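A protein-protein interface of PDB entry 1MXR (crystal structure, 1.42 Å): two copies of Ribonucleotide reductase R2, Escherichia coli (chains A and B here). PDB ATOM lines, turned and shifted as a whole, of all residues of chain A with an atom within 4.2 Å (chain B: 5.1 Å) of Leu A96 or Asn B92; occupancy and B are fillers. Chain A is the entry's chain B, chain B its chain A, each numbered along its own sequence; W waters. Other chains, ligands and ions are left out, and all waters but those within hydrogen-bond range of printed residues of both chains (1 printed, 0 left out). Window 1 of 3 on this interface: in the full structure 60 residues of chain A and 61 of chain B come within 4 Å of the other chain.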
ATOM      1  N   PRO A  91       8.165 -21.463  19.637  1.00  0.00           N
ATOM      2  CA  PRO A  91       7.791 -20.079  19.327  1.00  0.00           C
ATOM      3  C   PRO A  91       6.262 -19.959  19.415  1.00  0.00           C
ATOM      4  O   PRO A  91       5.721 -18.961  19.918  1.00  0.00           O
ATOM      5  CB  PRO A  91       8.327 -19.897  17.900  1.00  0.00           C
ATOM      6  CG  PRO A  91       9.529 -20.755  17.875  1.00  0.00           C
ATOM      7  CD  PRO A  91       9.052 -22.020  18.613  1.00  0.00           C
ATOM      8  N   ASN A  92       5.546 -21.011  19.013  1.00  0.00           N
ATOM      9  CA  ASN A  92       4.105 -20.977  19.108  1.00  0.00           C
ATOM     10  C   ASN A  92       3.619 -20.993  20.553  1.00  0.00           C
ATOM     11  O   ASN A  92       2.851 -20.099  20.941  1.00  0.00           O
ATOM     12  CB  ASN A  92       3.435 -22.138  18.350  1.00  0.00           C
ATOM     13  CG  ASN A  92       3.358 -21.905  16.835  1.00  0.00           C
ATOM     14  OD1 ASN A  92       3.272 -20.775  16.368  1.00  0.00           O
ATOM     15  ND2 ASN A  92       3.375 -22.991  16.089  1.00  0.00           N
ATOM     16  N   ALA A  94       5.213 -20.416  23.400  1.00  0.00           N
ATOM     17  CA  ALA A  94       5.744 -19.332  24.216  1.00  0.00           C
ATOM     18  C   ALA A  94       5.478 -17.913  23.738  1.00  0.00           C
ATOM     19  O   ALA A  94       5.260 -17.003  24.559  1.00  0.00           O
ATOM     20  CB  ALA A  94       7.240 -19.535  24.397  1.00  0.00           C
ATOM     21  N   LEU A  95       5.404 -17.706  22.421  1.00  0.00           N
ATOM     22  CA  LEU A  95       5.227 -16.327  21.969  1.00  0.00           C
ATOM     23  C   LEU A  95       3.849 -15.922  21.561  1.00  0.00           C
ATOM     24  O   LEU A  95       3.420 -14.801  21.837  1.00  0.00           O
ATOM     25  CB  LEU A  95       6.229 -16.044  20.830  1.00  0.00           C
ATOM     26  CG  LEU A  95       7.696 -16.364  21.137  1.00  0.00           C
ATOM     27  CD1 LEU A  95       8.558 -16.082  19.881  1.00  0.00           C
ATOM     28  CD2 LEU A  95       8.215 -15.542  22.346  1.00  0.00           C
ATOM     29  N   LEU A  96       3.102 -16.851  20.952  1.00  0.00           N
ATOM     30  CA  LEU A  96       1.770 -16.486  20.480  1.00  0.00           C
ATOM     31  C   LEU A  96       0.875 -15.888  21.528  1.00  0.00           C
ATOM     32  O   LEU A  96       0.130 -14.938  21.261  1.00  0.00           O
ATOM     33  CB  LEU A  96       0.993 -17.660  19.842  1.00  0.00           C
ATOM     34  CG  LEU A  96       1.492 -18.203  18.518  1.00  0.00           C
ATOM     35  CD1 LEU A  96       0.536 -19.329  18.072  1.00  0.00           C
ATOM     36  CD2 LEU A  96       1.530 -17.064  17.435  1.00  0.00           C
ATOM     37  N   PRO A  97       0.902 -16.425  22.761  1.00  0.00           N
ATOM     38  CA  PRO A  97       0.015 -15.837  23.772  1.00  0.00           C
ATOM     39  C   PRO A  97       0.324 -14.395  24.168  1.00  0.00           C
ATOM     40  O   PRO A  97      -0.489 -13.748  24.816  1.00  0.00           O
ATOM     41  CB  PRO A  97       0.156 -16.800  24.977  1.00  0.00           C
ATOM     42  CG  PRO A  97       0.598 -18.099  24.334  1.00  0.00           C
ATOM     43  CD  PRO A  97       1.562 -17.657  23.237  1.00  0.00           C
ATOM     44  N   LEU A  98       1.489 -13.892  23.750  1.00  0.00           N
ATOM     45  CA  LEU A  98       1.945 -12.556  24.140  1.00  0.00           C
ATOM     46  C   LEU A  98       1.980 -11.557  23.002  1.00  0.00           C
ATOM     47  O   LEU A  98       2.242 -10.392  23.252  1.00  0.00           O
ATOM     48  CB  LEU A  98       3.349 -12.648  24.731  1.00  0.00           C
ATOM     49  CG  LEU A  98       3.514 -13.486  26.011  1.00  0.00           C
ATOM     50  CD1 LEU A  98       4.988 -13.586  26.365  1.00  0.00           C
ATOM     51  CD2 LEU A  98       2.705 -12.866  27.138  1.00  0.00           C
ATOM     52  N   ILE A  99       1.689 -11.986  21.787  1.00  0.00           N
ATOM     53  CA  ILE A  99       1.816 -11.092  20.624  1.00  0.00           C
ATOM     54  C   ILE A  99       0.567 -10.256  20.385  1.00  0.00           C
ATOM     55  O   ILE A  99      -0.564 -10.739  20.510  1.00  0.00           O
ATOM     56  CB  ILE A  99       2.180 -11.927  19.390  1.00  0.00           C
ATOM     57  CG1 ILE A  99       3.622 -12.412  19.496  1.00  0.00           C
ATOM     58  CG2 ILE A  99       2.035 -11.075  18.116  1.00  0.00           C
ATOM     59  CD1 ILE A  99       3.939 -13.539  18.534  1.00  0.00           C
ATOM     60  N   GLU A 105       2.376 -12.089  14.790  1.00  0.00           N
ATOM     61  CA  GLU A 105       1.686 -13.334  15.116  1.00  0.00           C
ATOM     62  C   GLU A 105       1.839 -14.326  13.983  1.00  0.00           C
ATOM     63  O   GLU A 105       2.224 -15.484  14.197  1.00  0.00           O
ATOM     64  CB  GLU A 105       0.192 -13.086  15.330  1.00  0.00           C
ATOM     65  CG  GLU A 105      -0.543 -14.332  15.817  1.00  0.00           C
ATOM     66  CD  GLU A 105      -2.046 -14.141  15.875  1.00  0.00           C
ATOM     67  OE1 GLU A 105      -2.712 -13.931  14.825  1.00  0.00           O
ATOM     68  OE2 GLU A 105      -2.596 -14.205  16.984  1.00  0.00           O
ATOM     69  N   VAL A 108       5.440 -15.596  13.550  1.00  0.00           N
ATOM     70  CA  VAL A 108       5.797 -16.664  14.490  1.00  0.00           C
ATOM     71  C   VAL A 108       5.224 -18.024  14.069  1.00  0.00           C
ATOM     72  O   VAL A 108       5.928 -19.032  14.160  1.00  0.00           O
ATOM     73  CB  VAL A 108       5.353 -16.268  15.886  1.00  0.00           C
ATOM     74  CG1 VAL A 108       5.367 -17.483  16.852  1.00  0.00           C
ATOM     75  CG2 VAL A 108       6.324 -15.221  16.427  1.00  0.00           C
ATOM     76  N   GLU A 109       3.969 -18.047  13.604  1.00  0.00           N
ATOM     77  CA  GLU A 109       3.389 -19.327  13.168  1.00  0.00           C
ATOM     78  C   GLU A 109       4.031 -19.876  11.910  1.00  0.00           C
ATOM     79  O   GLU A 109       4.099 -21.088  11.701  1.00  0.00           O
ATOM     80  CB  GLU A 109       1.886 -19.176  12.969  1.00  0.00           C
ATOM     81  CG  GLU A 109       1.188 -18.689  14.287  1.00  0.00           C
ATOM     82  CD  GLU A 109      -0.298 -18.849  14.226  1.00  0.00           C
ATOM     83  OE1 GLU A 109      -0.768 -19.998  14.422  1.00  0.00           O
ATOM     84  OE2 GLU A 109      -1.026 -17.875  13.980  1.00  0.00           O
ATOM     85  N   GLY B  88      -6.411 -19.565  12.715  1.00  0.00           N
ATOM     86  CA  GLY B  88      -4.978 -19.430  12.520  1.00  0.00           C
ATOM     87  C   GLY B  88      -4.227 -19.598  13.835  1.00  0.00           C
ATOM     88  O   GLY B  88      -3.201 -20.319  13.935  1.00  0.00           O
ATOM     89  N   ARG B  89      -4.748 -18.973  14.880  1.00  0.00           N
ATOM     90  CA  ARG B  89      -4.058 -19.029  16.174  1.00  0.00           C
ATOM     91  C   ARG B  89      -4.507 -20.118  17.153  1.00  0.00           C
ATOM     92  O   ARG B  89      -3.663 -20.685  17.869  1.00  0.00           O
ATOM     93  CB  ARG B  89      -4.185 -17.658  16.907  1.00  0.00           C
ATOM     94  CG  ARG B  89      -5.608 -17.257  17.328  1.00  0.00           C
ATOM     95  CD  ARG B  89      -5.669 -15.858  17.925  1.00  0.00           C
ATOM     96  NE  ARG B  89      -5.269 -14.846  16.934  1.00  0.00           N
ATOM     97  CZ  ARG B  89      -6.122 -14.089  16.248  1.00  0.00           C
ATOM     98  NH1 ARG B  89      -7.449 -14.140  16.419  1.00  0.00           N
ATOM     99  NH2 ARG B  89      -5.603 -13.328  15.289  1.00  0.00           N
ATOM    100  N   SER B  90      -5.798 -20.416  17.145  1.00  0.00           N
ATOM    101  CA  SER B  90      -6.359 -21.252  18.190  1.00  0.00           C
ATOM    102  C   SER B  90      -5.877 -22.695  18.289  1.00  0.00           C
ATOM    103  O   SER B  90      -5.652 -23.189  19.393  1.00  0.00           O
ATOM    104  CB  SER B  90      -7.886 -21.156  18.158  1.00  0.00           C
ATOM    105  OG  SER B  90      -8.263 -19.776  18.367  1.00  0.00           O
ATOM    106  N   PRO B  91      -5.671 -23.404  17.184  1.00  0.00           N
ATOM    107  CA  PRO B  91      -5.193 -24.781  17.354  1.00  0.00           C
ATOM    108  C   PRO B  91      -3.826 -24.767  18.026  1.00  0.00           C
ATOM    109  O   PRO B  91      -3.517 -25.656  18.833  1.00  0.00           O
ATOM    110  CB  PRO B  91      -5.163 -25.323  15.913  1.00  0.00           C
ATOM    111  CG  PRO B  91      -6.276 -24.533  15.238  1.00  0.00           C
ATOM    112  CD  PRO B  91      -6.052 -23.134  15.781  1.00  0.00           C
ATOM    113  N   ASN B  92      -3.005 -23.769  17.740  1.00  0.00           N
ATOM    114  CA  ASN B  92      -1.676 -23.674  18.359  1.00  0.00           C
ATOM    115  C   ASN B  92      -1.734 -23.233  19.828  1.00  0.00           C
ATOM    116  O   ASN B  92      -1.029 -23.788  20.678  1.00  0.00           O
ATOM    117  CB  ASN B  92      -0.784 -22.702  17.586  1.00  0.00           C
ATOM    118  CG  ASN B  92      -0.157 -23.333  16.373  1.00  0.00           C
ATOM    119  OD1 ASN B  92       0.082 -24.522  16.340  1.00  0.00           O
ATOM    120  ND2 ASN B  92       0.196 -22.508  15.380  1.00  0.00           N
ATOM    121  N   VAL B  93      -2.567 -22.276  20.175  1.00  0.00           N
ATOM    122  CA  VAL B  93      -2.588 -21.848  21.570  1.00  0.00           C
ATOM    123  C   VAL B  93      -3.403 -22.782  22.461  1.00  0.00           C
ATOM    124  O   VAL B  93      -3.057 -22.966  23.620  1.00  0.00           O
ATOM    125  CB  VAL B  93      -3.084 -20.351  21.765  1.00  0.00           C
ATOM    126  CG1 VAL B  93      -2.108 -19.430  21.071  1.00  0.00           C
ATOM    127  CG2 VAL B  93      -4.454 -20.122  21.206  1.00  0.00           C
ATOM    128  N   ALA B  94      -4.420 -23.438  21.920  1.00  0.00           N
ATOM    129  CA  ALA B  94      -5.294 -24.293  22.726  1.00  0.00           C
ATOM    130  C   ALA B  94      -5.009 -25.768  22.649  1.00  0.00           C
ATOM    131  O   ALA B  94      -5.148 -26.456  23.677  1.00  0.00           O
ATOM    132  CB  ALA B  94      -6.765 -24.040  22.340  1.00  0.00           C
ATOM    133  N   LEU B  95      -4.578 -26.270  21.501  1.00  0.00           N
ATOM    134  CA  LEU B  95      -4.355 -27.716  21.372  1.00  0.00           C
ATOM    135  C   LEU B  95      -2.933 -28.120  21.514  1.00  0.00           C
ATOM    136  O   LEU B  95      -2.622 -29.095  22.163  1.00  0.00           O
ATOM    137  CB  LEU B  95      -4.924 -28.211  20.019  1.00  0.00           C
ATOM    138  CG  LEU B  95      -6.377 -27.806  19.743  1.00  0.00           C
ATOM    139  CD1 LEU B  95      -6.837 -28.353  18.412  1.00  0.00           C
ATOM    140  CD2 LEU B  95      -7.300 -28.387  20.831  1.00  0.00           C
ATOM    141  N   LEU B  96      -2.015 -27.363  20.936  1.00  0.00           N
ATOM    142  CA  LEU B  96      -0.632 -27.717  20.984  1.00  0.00           C
ATOM    143  C   LEU B  96      -0.058 -28.010  22.390  1.00  0.00           C
ATOM    144  O   LEU B  96       0.682 -28.982  22.560  1.00  0.00           O
ATOM    145  CB  LEU B  96       0.145 -26.634  20.196  1.00  0.00           C
ATOM    146  CG  LEU B  96       1.636 -26.732  20.093  1.00  0.00           C
ATOM    147  CD1 LEU B  96       2.044 -28.049  19.378  1.00  0.00           C
ATOM    148  CD2 LEU B  96       2.086 -25.510  19.266  1.00  0.00           C
ATOM    149  N   PRO B  97      -0.441 -27.240  23.425  1.00  0.00           N
ATOM    150  CA  PRO B  97       0.113 -27.519  24.755  1.00  0.00           C
ATOM    151  C   PRO B  97      -0.367 -28.839  25.399  1.00  0.00           C
ATOM    152  O   PRO B  97       0.159 -29.273  26.431  1.00  0.00           O
ATOM    153  CB  PRO B  97      -0.348 -26.307  25.577  1.00  0.00           C
ATOM    154  CG  PRO B  97      -0.531 -25.243  24.570  1.00  0.00           C
ATOM    155  CD  PRO B  97      -1.170 -25.965  23.431  1.00  0.00           C
ATOM    156  N   VAL B 108      -1.245 -30.403  13.922  1.00  0.00           N
ATOM    157  CA  VAL B 108      -1.886 -29.215  14.422  1.00  0.00           C
ATOM    158  C   VAL B 108      -1.123 -27.954  13.982  1.00  0.00           C
ATOM    159  O   VAL B 108      -1.770 -26.969  13.573  1.00  0.00           O
ATOM    160  CB  VAL B 108      -2.039 -29.329  15.938  1.00  0.00           C
ATOM    161  CG1 VAL B 108      -2.417 -27.965  16.555  1.00  0.00           C
ATOM    162  CG2 VAL B 108      -3.153 -30.325  16.210  1.00  0.00           C
ATOM    163  N   GLU B 109       0.203 -27.960  14.042  1.00  0.00           N
ATOM    164  CA  GLU B 109       0.960 -26.783  13.632  1.00  0.00           C
ATOM    165  C   GLU B 109       0.848 -26.562  12.117  1.00  0.00           C
ATOM    166  O   GLU B 109       0.905 -25.393  11.670  1.00  0.00           O
ATOM    167  CB  GLU B 109       2.420 -26.941  14.048  1.00  0.00           C
ATOM    168  CG  GLU B 109       2.556 -27.050  15.557  1.00  0.00           C
ATOM    169  CD  GLU B 109       3.962 -26.826  16.021  1.00  0.00           C
ATOM    170  OE1 GLU B 109       4.671 -27.813  16.252  1.00  0.00           O
ATOM    171  OE2 GLU B 109       4.382 -25.653  16.151  1.00  0.00           O
ATOM    172  N   ALA B 112      -2.803 -25.186  11.543  1.00  0.00           N
ATOM    173  CA  ALA B 112      -2.845 -23.765  11.914  1.00  0.00           C
ATOM    174  C   ALA B 112      -2.129 -22.912  10.872  1.00  0.00           C
ATOM    175  O   ALA B 112      -2.627 -21.826  10.496  1.00  0.00           O
ATOM    176  CB  ALA B 112      -2.205 -23.577  13.286  1.00  0.00           C
HETATM  177  O   HOH W   1       2.303 -23.101  13.111  1.00  0.00           O
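Of the printed residues of chain B, Asn A92 touches Asn B92, Leu B96 and Glu B109.
Leu A96 touches just these residues of chain B: Asn B92 (3.7 Å) and Val B93 (3.8 Å).
Of the printed residues of chain A, Arg B89 touches Glu A105 and Glu A109.
Of chain A, only Asn A92, Leu A96 and Glu A109 come within 4 Å of Asn B92.
Of the printed residues of chain A, Glu B109 touches Asn A92 (2.8 Å).
The nearest printed residue of chain A that does not touch Asn B92 is Val A108 (6.8 Å).
Water W1 lies within hydrogen-bond range of the backbone carbonyl oxygen (O) of Glu A109, the backbone carbonyl oxygen (O) of Glu B109, the side-chain amide nitrogen (ND2) of Asn B92 and the side-chain amide nitrogen (ND2) of Asn A92.
Along chain B the printed residues that touch a printed residue of chain A span positions 88 to 109.
Of the 11 printed residues of chain A, 4 touch a printed residue of chain B.
Asn B92 touches its own counterpart, Asn A92.
Asn A92 touches Leu B96, and with the chains exchanged Leu A96 touches Asn B92.
Asn A92 touches Glu B109, and with the chains exchanged Glu A109 touches Asn B92.
8 positions are printed for both chains.
Of the 9 pairs that touch across the chains among the printed residues, 5 have their exchanged pair printed and touching as well.
Among the printed residues, pairs that only touch across the chains: Asn A92 with Leu B96 (3.7 Å), Leu A96 with Asn B92 (3.7 Å), Leu A96 with Val B93 (3.8 Å) and Glu A109 with Arg B89 (3.9 Å).
O of Pro B91 is in hydrogen-bond range of N of Leu B96 (3.1 Å).
OE1 of Glu A109 sits at hydrogen-bond distance from ND2 of Asn B92 (2.9 Å).
OE2 of Glu B109 is in hydrogen-bond range of ND2 of Asn A92, 2.8 Å away.
The backbone carbonyl oxygen (O) of Gly B88 sits close to the side-chain carboxylate (OE1) of Glu A109, 2.5 Å away.
The guanidinium group (NE) of Arg B89 is in salt-bridge range of the side-chain carboxylate (OE2) of Glu A105, at 2.7 Å.
The side-chain amide nitrogen (ND2) of Asn B92 sits close to the side-chain amide nitrogen (ND2) of Asn A92, at 3.3 Å.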
